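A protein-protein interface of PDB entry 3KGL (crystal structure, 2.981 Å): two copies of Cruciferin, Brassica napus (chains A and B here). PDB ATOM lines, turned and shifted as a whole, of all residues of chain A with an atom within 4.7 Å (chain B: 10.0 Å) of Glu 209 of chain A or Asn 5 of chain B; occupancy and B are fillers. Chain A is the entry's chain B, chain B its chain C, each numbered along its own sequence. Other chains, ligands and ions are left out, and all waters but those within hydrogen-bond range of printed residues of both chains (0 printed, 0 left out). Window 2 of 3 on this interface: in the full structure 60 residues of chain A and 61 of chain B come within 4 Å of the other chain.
The side-chain carboxylate (OD2) of Asp 10 of chain B is in salt-bridge range of the guanidinium group (NH1) of Arg 211 of chain A. The guanidinium group (NH2) of Arg 211 of chain A lies close to the side-chain amide nitrogen (NE2) of Gln 8 of chain B, at 2.9 Å. OD2 of Asp 189 of chain A is in hydrogen-bond range of N of Glu 6 of chain B (2.9 Å). OD2 of Asp 189 of chain A lies close to O of Pro 4 of chain B, 3.3 Å away. The side-chain carboxylate (OD2) of Asp 189 of chain A lies within hydrogen-bond range of the backbone NH (N) of Cys 7 of chain B.
The side-chain sulfur of Cys 40 of chain B is disulfide-bonded to the side-chain sulfur of Cys 7 of chain B (2.1 Å). The side-chain amide nitrogen of Asn 191 of chain A sits at hydrogen-bond distance from the side-chain carboxylate of Asp 189 of chain A, 2.7 Å away.
C of Asn 5 of chain B touches OD2 of Asp 189 of chain A, at 3.2 Å. Asn 191 of chain A touches Pro 4 of chain B (ND2 to O, 3.8 Å). Asn 5 of chain B touches Asn 191 of chain A. Gln 8 of chain B touches Ile 208 of chain A. Glu 209 of chain A touches Asn 5 of chain B (O to OD1, 3.9 Å).
Of the printed residues of chain B, Asn 191 of chain A touches Pro 4 (3.8 Å) and Asn 5 (3.6 Å). Of the printed residues of chain B, Glu 209 of chain A touches Asn 5 (3.9 Å). Gly 210 of chain A touches none of the printed residues of chain B. Asn 5 of chain B touches just these residues of chain A: Asp 189, Asn 191 and Glu 209. Of the printed residues of chain A, Asp 10 of chain B touches Arg 211 (3.8 Å). Cys 40 of chain B touches none of the printed residues of chain A. The nearest residue of chain B that does not touch Glu 209 of chain A is Gln 8 of chain B (4.7 Å). The nearest printed residue of chain B that does not touch Asn 191 of chain A is Gln 8 of chain B (5.8 Å).
Hydrophobic or aromatic side chains of chain A within 4 Å of the printed part of chain B: Ile 208. Printed residues of chain B that touch a printed residue of chain A: Pro 4, Asn 5, Glu 6, Cys 7, Gln 8 and Asp 10. Among the printed residues, 10 pairs touch across the chains. Among the printed residues, Asp or Glu carboxylates within 4 Å of a Lys or Arg side-chain nitrogen of the other chain: Arg 211 of chain A with Asp 10 of chain B (3.8 Å).
No position is printed for both chains.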
ATOM      1  N   HIS A  34       8.362 -26.245 -29.966  1.00  0.00           N
ATOM      2  CA  HIS A  34       7.636 -27.031 -28.977  1.00  0.00           C
ATOM      3  C   HIS A  34       6.632 -27.958 -29.674  1.00  0.00           C
ATOM      4  O   HIS A  34       6.073 -28.868 -29.064  1.00  0.00           O
ATOM      5  CB  HIS A  34       6.918 -26.129 -27.974  1.00  0.00           C
ATOM      6  CG  HIS A  34       7.837 -25.298 -27.140  1.00  0.00           C
ATOM      7  ND1 HIS A  34       7.552 -23.993 -26.797  1.00  0.00           N
ATOM      8  CD2 HIS A  34       9.038 -25.581 -26.582  1.00  0.00           C
ATOM      9  CE1 HIS A  34       8.535 -23.510 -26.058  1.00  0.00           C
ATOM     10  NE2 HIS A  34       9.448 -24.453 -25.913  1.00  0.00           N
ATOM     11  N   ASP A 189      20.766 -25.759 -24.003  1.00  0.00           N
ATOM     12  CA  ASP A 189      19.341 -25.709 -23.743  1.00  0.00           C
ATOM     13  C   ASP A 189      18.596 -26.238 -24.945  1.00  0.00           C
ATOM     14  O   ASP A 189      19.145 -26.318 -26.032  1.00  0.00           O
ATOM     15  CB  ASP A 189      18.951 -24.245 -23.580  1.00  0.00           C
ATOM     16  CG  ASP A 189      17.911 -24.037 -22.531  1.00  0.00           C
ATOM     17  OD1 ASP A 189      17.106 -23.109 -22.683  1.00  0.00           O
ATOM     18  OD2 ASP A 189      17.909 -24.792 -21.547  1.00  0.00           O
ATOM     19  N   ASN A 191      16.243 -24.753 -26.554  1.00  0.00           N
ATOM     20  CA  ASN A 191      15.605 -23.659 -27.284  1.00  0.00           C
ATOM     21  C   ASN A 191      16.584 -23.012 -28.286  1.00  0.00           C
ATOM     22  O   ASN A 191      17.804 -23.131 -28.148  1.00  0.00           O
ATOM     23  CB  ASN A 191      15.041 -22.587 -26.341  1.00  0.00           C
ATOM     24  CG  ASN A 191      14.280 -23.165 -25.165  1.00  0.00           C
ATOM     25  OD1 ASN A 191      13.072 -22.980 -25.043  1.00  0.00           O
ATOM     26  ND2 ASN A 191      14.991 -23.837 -24.276  1.00  0.00           N
ATOM     27  N   TRP A 207       9.594 -16.872 -28.479  1.00  0.00           N
ATOM     28  CA  TRP A 207       9.760 -18.270 -28.895  1.00  0.00           C
ATOM     29  C   TRP A 207      10.241 -19.203 -27.788  1.00  0.00           C
ATOM     30  O   TRP A 207      10.271 -20.405 -27.993  1.00  0.00           O
ATOM     31  CB  TRP A 207      10.728 -18.383 -30.073  1.00  0.00           C
ATOM     32  CG  TRP A 207      12.119 -18.006 -29.719  1.00  0.00           C
ATOM     33  CD1 TRP A 207      13.150 -18.849 -29.427  1.00  0.00           C
ATOM     34  CD2 TRP A 207      12.639 -16.675 -29.603  1.00  0.00           C
ATOM     35  NE1 TRP A 207      14.286 -18.126 -29.140  1.00  0.00           N
ATOM     36  CE2 TRP A 207      13.998 -16.789 -29.236  1.00  0.00           C
ATOM     37  CE3 TRP A 207      12.087 -15.399 -29.767  1.00  0.00           C
ATOM     38  CZ2 TRP A 207      14.811 -15.678 -29.032  1.00  0.00           C
ATOM     39  CZ3 TRP A 207      12.896 -14.296 -29.567  1.00  0.00           C
ATOM     40  CH2 TRP A 207      14.245 -14.442 -29.200  1.00  0.00           C
ATOM     41  N   ILE A 208      10.615 -18.642 -26.633  1.00  0.00           N
ATOM     42  CA  ILE A 208      11.035 -19.405 -25.445  1.00  0.00           C
ATOM     43  C   ILE A 208      10.126 -19.158 -24.244  1.00  0.00           C
ATOM     44  O   ILE A 208      10.196 -18.093 -23.618  1.00  0.00           O
ATOM     45  CB  ILE A 208      12.399 -18.958 -24.953  1.00  0.00           C
ATOM     46  CG1 ILE A 208      13.433 -19.027 -26.063  1.00  0.00           C
ATOM     47  CG2 ILE A 208      12.816 -19.795 -23.793  1.00  0.00           C
ATOM     48  CD1 ILE A 208      14.759 -18.465 -25.634  1.00  0.00           C
ATOM     49  N   GLU A 209       9.301 -20.137 -23.889  1.00  0.00           N
ATOM     50  CA  GLU A 209       8.346 -19.926 -22.801  1.00  0.00           C
ATOM     51  C   GLU A 209       9.029 -19.600 -21.466  1.00  0.00           C
ATOM     52  O   GLU A 209      10.214 -19.886 -21.253  1.00  0.00           O
ATOM     53  CB  GLU A 209       7.374 -21.106 -22.664  1.00  0.00           C
ATOM     54  CG  GLU A 209       7.944 -22.319 -21.955  1.00  0.00           C
ATOM     55  CD  GLU A 209       7.068 -23.546 -22.126  1.00  0.00           C
ATOM     56  OE1 GLU A 209       6.290 -23.570 -23.108  1.00  0.00           O
ATOM     57  OE2 GLU A 209       7.163 -24.480 -21.289  1.00  0.00           O
ATOM     58  N   GLY A 210       8.277 -18.972 -20.573  1.00  0.00           N
ATOM     59  CA  GLY A 210       8.834 -18.560 -19.304  1.00  0.00           C
ATOM     60  C   GLY A 210       9.513 -17.211 -19.400  1.00  0.00           C
ATOM     61  O   GLY A 210      10.146 -16.758 -18.447  1.00  0.00           O
ATOM     62  N   ARG A 211       9.381 -16.559 -20.550  1.00  0.00           N
ATOM     63  CA  ARG A 211       9.997 -15.247 -20.733  1.00  0.00           C
ATOM     64  C   ARG A 211       9.303 -14.129 -19.956  1.00  0.00           C
ATOM     65  O   ARG A 211       9.949 -13.230 -19.421  1.00  0.00           O
ATOM     66  CB  ARG A 211      10.123 -14.890 -22.220  1.00  0.00           C
ATOM     67  CG  ARG A 211      11.458 -15.319 -22.803  1.00  0.00           C
ATOM     68  CD  ARG A 211      12.651 -14.496 -22.262  1.00  0.00           C
ATOM     69  NE  ARG A 211      12.461 -14.048 -20.881  1.00  0.00           N
ATOM     70  CZ  ARG A 211      13.414 -14.004 -19.954  1.00  0.00           C
ATOM     71  NH1 ARG A 211      13.113 -13.587 -18.740  1.00  0.00           N
ATOM     72  NH2 ARG A 211      14.653 -14.396 -20.226  1.00  0.00           N
ATOM     73  N   GLN B   1      12.555 -23.121 -14.869  1.00  0.00           N
ATOM     74  CA  GLN B   1      13.829 -23.112 -14.158  1.00  0.00           C
ATOM     75  C   GLN B   1      14.595 -24.429 -14.339  1.00  0.00           C
ATOM     76  O   GLN B   1      15.771 -24.520 -13.978  1.00  0.00           O
ATOM     77  CB  GLN B   1      13.616 -22.828 -12.663  1.00  0.00           C
ATOM     78  CG  GLN B   1      12.748 -21.608 -12.350  1.00  0.00           C
ATOM     79  CD  GLN B   1      11.263 -21.938 -12.271  1.00  0.00           C
ATOM     80  OE1 GLN B   1      10.858 -23.106 -12.378  1.00  0.00           O
ATOM     81  NE2 GLN B   1      10.442 -20.905 -12.076  1.00  0.00           N
ATOM     82  N   GLN B   2      13.928 -25.435 -14.910  1.00  0.00           N
ATOM     83  CA  GLN B   2      14.492 -26.788 -15.049  1.00  0.00           C
ATOM     84  C   GLN B   2      14.199 -27.448 -16.412  1.00  0.00           C
ATOM     85  O   GLN B   2      13.277 -27.037 -17.126  1.00  0.00           O
ATOM     86  CB  GLN B   2      13.989 -27.678 -13.906  1.00  0.00           C
ATOM     87  CG  GLN B   2      14.443 -27.215 -12.524  1.00  0.00           C
ATOM     88  CD  GLN B   2      13.467 -27.581 -11.425  1.00  0.00           C
ATOM     89  OE1 GLN B   2      12.296 -27.199 -11.466  1.00  0.00           O
ATOM     90  NE2 GLN B   2      13.951 -28.313 -10.424  1.00  0.00           N
ATOM     91  N   PHE B   3      14.999 -28.461 -16.761  1.00  0.00           N
ATOM     92  CA  PHE B   3      14.932 -29.171 -18.059  1.00  0.00           C
ATOM     93  C   PHE B   3      13.540 -29.107 -18.720  1.00  0.00           C
ATOM     94  O   PHE B   3      12.520 -29.200 -18.042  1.00  0.00           O
ATOM     95  CB  PHE B   3      15.409 -30.627 -17.872  1.00  0.00           C
ATOM     96  CG  PHE B   3      15.716 -31.362 -19.155  1.00  0.00           C
ATOM     97  CD1 PHE B   3      16.888 -31.111 -19.856  1.00  0.00           C
ATOM     98  CD2 PHE B   3      14.853 -32.339 -19.637  1.00  0.00           C
ATOM     99  CE1 PHE B   3      17.180 -31.799 -21.028  1.00  0.00           C
ATOM    100  CE2 PHE B   3      15.137 -33.031 -20.806  1.00  0.00           C
ATOM    101  CZ  PHE B   3      16.305 -32.760 -21.501  1.00  0.00           C
ATOM    102  N   PRO B   4      13.488 -28.923 -20.049  1.00  0.00           N
ATOM    103  CA  PRO B   4      14.606 -28.757 -20.982  1.00  0.00           C
ATOM    104  C   PRO B   4      14.936 -27.283 -21.161  1.00  0.00           C
ATOM    105  O   PRO B   4      15.527 -26.915 -22.174  1.00  0.00           O
ATOM    106  CB  PRO B   4      14.041 -29.295 -22.304  1.00  0.00           C
ATOM    107  CG  PRO B   4      12.533 -29.529 -22.056  1.00  0.00           C
ATOM    108  CD  PRO B   4      12.196 -28.874 -20.752  1.00  0.00           C
ATOM    109  N   ASN B   5      14.513 -26.456 -20.208  1.00  0.00           N
ATOM    110  CA  ASN B   5      14.850 -25.044 -20.202  1.00  0.00           C
ATOM    111  C   ASN B   5      15.895 -24.782 -19.124  1.00  0.00           C
ATOM    112  O   ASN B   5      15.888 -23.745 -18.456  1.00  0.00           O
ATOM    113  CB  ASN B   5      13.594 -24.204 -19.993  1.00  0.00           C
ATOM    114  CG  ASN B   5      12.657 -24.274 -21.182  1.00  0.00           C
ATOM    115  OD1 ASN B   5      11.870 -23.367 -21.421  1.00  0.00           O
ATOM    116  ND2 ASN B   5      12.753 -25.349 -21.944  1.00  0.00           N
ATOM    117  N   GLU B   6      16.793 -25.756 -18.993  1.00  0.00           N
ATOM    118  CA  GLU B   6      17.785 -25.830 -17.928  1.00  0.00           C
ATOM    119  C   GLU B   6      18.674 -24.614 -17.846  1.00  0.00           C
ATOM    120  O   GLU B   6      19.359 -24.417 -16.837  1.00  0.00           O
ATOM    121  CB  GLU B   6      18.664 -27.078 -18.104  1.00  0.00           C
ATOM    122  CG  GLU B   6      18.478 -27.797 -19.442  1.00  0.00           C
ATOM    123  CD  GLU B   6      19.580 -28.801 -19.721  1.00  0.00           C
ATOM    124  OE1 GLU B   6      19.440 -29.596 -20.681  1.00  0.00           O
ATOM    125  OE2 GLU B   6      20.590 -28.788 -18.983  1.00  0.00           O
ATOM    126  N   CYS B   7      18.677 -23.813 -18.910  1.00  0.00           N
ATOM    127  CA  CYS B   7      19.649 -22.729 -19.043  1.00  0.00           C
ATOM    128  C   CYS B   7      19.020 -21.351 -19.171  1.00  0.00           C
ATOM    129  O   CYS B   7      19.688 -20.395 -19.504  1.00  0.00           O
ATOM    130  CB  CYS B   7      20.641 -23.002 -20.180  1.00  0.00           C
ATOM    131  SG  CYS B   7      21.887 -24.269 -19.786  1.00  0.00           S
ATOM    132  N   GLN B   8      17.734 -21.243 -18.881  1.00  0.00           N
ATOM    133  CA  GLN B   8      17.128 -19.936 -18.717  1.00  0.00           C
ATOM    134  C   GLN B   8      17.487 -19.409 -17.337  1.00  0.00           C
ATOM    135  O   GLN B   8      16.610 -19.206 -16.496  1.00  0.00           O
ATOM    136  CB  GLN B   8      15.612 -20.031 -18.856  1.00  0.00           C
ATOM    137  CG  GLN B   8      14.918 -18.688 -18.945  1.00  0.00           C
ATOM    138  CD  GLN B   8      14.717 -18.254 -20.365  1.00  0.00           C
ATOM    139  OE1 GLN B   8      15.223 -18.892 -21.292  1.00  0.00           O
ATOM    140  NE2 GLN B   8      13.962 -17.177 -20.559  1.00  0.00           N
ATOM    141  N   LEU B   9      18.783 -19.215 -17.098  1.00  0.00           N
ATOM    142  CA  LEU B   9      19.270 -18.628 -15.850  1.00  0.00           C
ATOM    143  C   LEU B   9      19.023 -17.129 -15.861  1.00  0.00           C
ATOM    144  O   LEU B   9      19.296 -16.473 -16.862  1.00  0.00           O
ATOM    145  CB  LEU B   9      20.765 -18.847 -15.716  1.00  0.00           C
ATOM    146  CG  LEU B   9      21.320 -20.242 -15.501  1.00  0.00           C
ATOM    147  CD1 LEU B   9      20.257 -21.077 -14.847  1.00  0.00           C
ATOM    148  CD2 LEU B   9      21.742 -20.834 -16.811  1.00  0.00           C
ATOM    149  N   ASP B  10      18.522 -16.575 -14.760  1.00  0.00           N
ATOM    150  CA  ASP B  10      18.344 -15.120 -14.678  1.00  0.00           C
ATOM    151  C   ASP B  10      19.211 -14.493 -13.573  1.00  0.00           C
ATOM    152  O   ASP B  10      19.191 -13.278 -13.376  1.00  0.00           O
ATOM    153  CB  ASP B  10      16.867 -14.729 -14.490  1.00  0.00           C
ATOM    154  CG  ASP B  10      15.987 -15.068 -15.707  1.00  0.00           C
ATOM    155  OD1 ASP B  10      16.524 -15.385 -16.796  1.00  0.00           O
ATOM    156  OD2 ASP B  10      14.741 -15.006 -15.569  1.00  0.00           O
ATOM    157  N   PRO B  36      20.697 -24.656 -10.544  1.00  0.00           N
ATOM    158  CA  PRO B  36      20.345 -24.318 -11.929  1.00  0.00           C
ATOM    159  C   PRO B  36      21.577 -23.972 -12.741  1.00  0.00           C
ATOM    160  O   PRO B  36      21.782 -24.485 -13.840  1.00  0.00           O
ATOM    161  CB  PRO B  36      19.490 -23.075 -11.768  1.00  0.00           C
ATOM    162  CG  PRO B  36      18.841 -23.257 -10.429  1.00  0.00           C
ATOM    163  CD  PRO B  36      19.784 -24.041  -9.569  1.00  0.00           C
ATOM    164  N   GLN B  37      22.400 -23.101 -12.180  1.00  0.00           N
ATOM    165  CA  GLN B  37      23.599 -22.631 -12.855  1.00  0.00           C
ATOM    166  C   GLN B  37      24.604 -23.751 -13.181  1.00  0.00           C
ATOM    167  O   GLN B  37      25.185 -23.764 -14.263  1.00  0.00           O
ATOM    168  CB  GLN B  37      24.210 -21.492 -12.036  1.00  0.00           C
ATOM    169  CG  GLN B  37      25.699 -21.519 -11.845  1.00  0.00           C
ATOM    170  CD  GLN B  37      26.153 -20.557 -10.752  1.00  0.00           C
ATOM    171  OE1 GLN B  37      25.380 -19.718 -10.266  1.00  0.00           O
ATOM    172  NE2 GLN B  37      27.411 -20.681 -10.354  1.00  0.00           N
ATOM    173  N   ARG B  39      23.744 -27.003 -13.324  1.00  0.00           N
ATOM    174  CA  ARG B  39      23.038 -28.010 -14.100  1.00  0.00           C
ATOM    175  C   ARG B  39      23.076 -27.578 -15.559  1.00  0.00           C
ATOM    176  O   ARG B  39      23.237 -28.393 -16.472  1.00  0.00           O
ATOM    177  CB  ARG B  39      21.592 -28.152 -13.610  1.00  0.00           C
ATOM    178  CG  ARG B  39      20.963 -29.521 -13.865  1.00  0.00           C
ATOM    179  CD  ARG B  39      19.492 -29.542 -13.490  1.00  0.00           C
ATOM    180  NE  ARG B  39      18.831 -28.295 -13.863  1.00  0.00           N
ATOM    181  CZ  ARG B  39      18.258 -27.462 -12.999  1.00  0.00           C
ATOM    182  NH1 ARG B  39      18.238 -27.756 -11.696  1.00  0.00           N
ATOM    183  NH2 ARG B  39      17.695 -26.341 -13.444  1.00  0.00           N
ATOM    184  N   CYS B  40      22.945 -26.273 -15.763  1.00  0.00           N
ATOM    185  CA  CYS B  40      23.052 -25.678 -17.082  1.00  0.00           C
ATOM    186  C   CYS B  40      24.358 -26.047 -17.784  1.00  0.00           C
ATOM    187  O   CYS B  40      24.358 -26.299 -18.982  1.00  0.00           O
ATOM    188  CB  CYS B  40      22.954 -24.165 -16.969  1.00  0.00           C
ATOM    189  SG  CYS B  40      23.206 -23.329 -18.529  1.00  0.00           S
ATOM    190  N   SER B  41      25.453 -26.080 -17.026  1.00  0.00           N
ATOM    191  CA  SER B  41      26.793 -26.371 -17.540  1.00  0.00           C
ATOM    192  C   SER B  41      27.051 -27.863 -17.732  1.00  0.00           C
ATOM    193  O   SER B  41      27.838 -28.266 -18.601  1.00  0.00           O
ATOM    194  CB  SER B  41      27.848 -25.833 -16.573  1.00  0.00           C
ATOM    195  OG  SER B  41      27.656 -24.459 -16.312  1.00  0.00           O
ATOM    196  N   ASP B 362      21.764 -14.220 -22.935  1.00  0.00           N
ATOM    197  CA  ASP B 362      21.304 -14.086 -24.298  1.00  0.00           C
ATOM    198  C   ASP B 362      20.128 -13.085 -24.361  1.00  0.00           C
ATOM    199  O   ASP B 362      19.744 -12.624 -25.433  1.00  0.00           O
ATOM    200  CB  ASP B 362      20.937 -15.464 -24.874  1.00  0.00           C
ATOM    201  CG  ASP B 362      19.799 -16.143 -24.121  1.00  0.00           C
ATOM    202  OD1 ASP B 362      19.748 -16.049 -22.879  1.00  0.00           O
ATOM    203  OD2 ASP B 362      18.946 -16.769 -24.782  1.00  0.00           O
ATOM    204  N   PHE B 384      27.439 -16.824 -22.836  1.00  0.00           N
ATOM    205  CA  PHE B 384      27.348 -15.742 -21.867  1.00  0.00           C
ATOM    206  C   PHE B 384      28.653 -14.941 -21.931  1.00  0.00           C
ATOM    207  O   PHE B 384      29.741 -15.507 -22.076  1.00  0.00           O
ATOM    208  CB  PHE B 384      27.111 -16.291 -20.451  1.00  0.00           C
ATOM    209  CG  PHE B 384      25.704 -16.776 -20.203  1.00  0.00           C
ATOM    210  CD1 PHE B 384      25.002 -17.470 -21.181  1.00  0.00           C
ATOM    211  CD2 PHE B 384      25.090 -16.559 -18.986  1.00  0.00           C
ATOM    212  CE1 PHE B 384      23.703 -17.921 -20.957  1.00  0.00           C
ATOM    213  CE2 PHE B 384      23.799 -17.009 -18.761  1.00  0.00           C
ATOM    214  CZ  PHE B 384      23.110 -17.692 -19.751  1.00  0.00           C
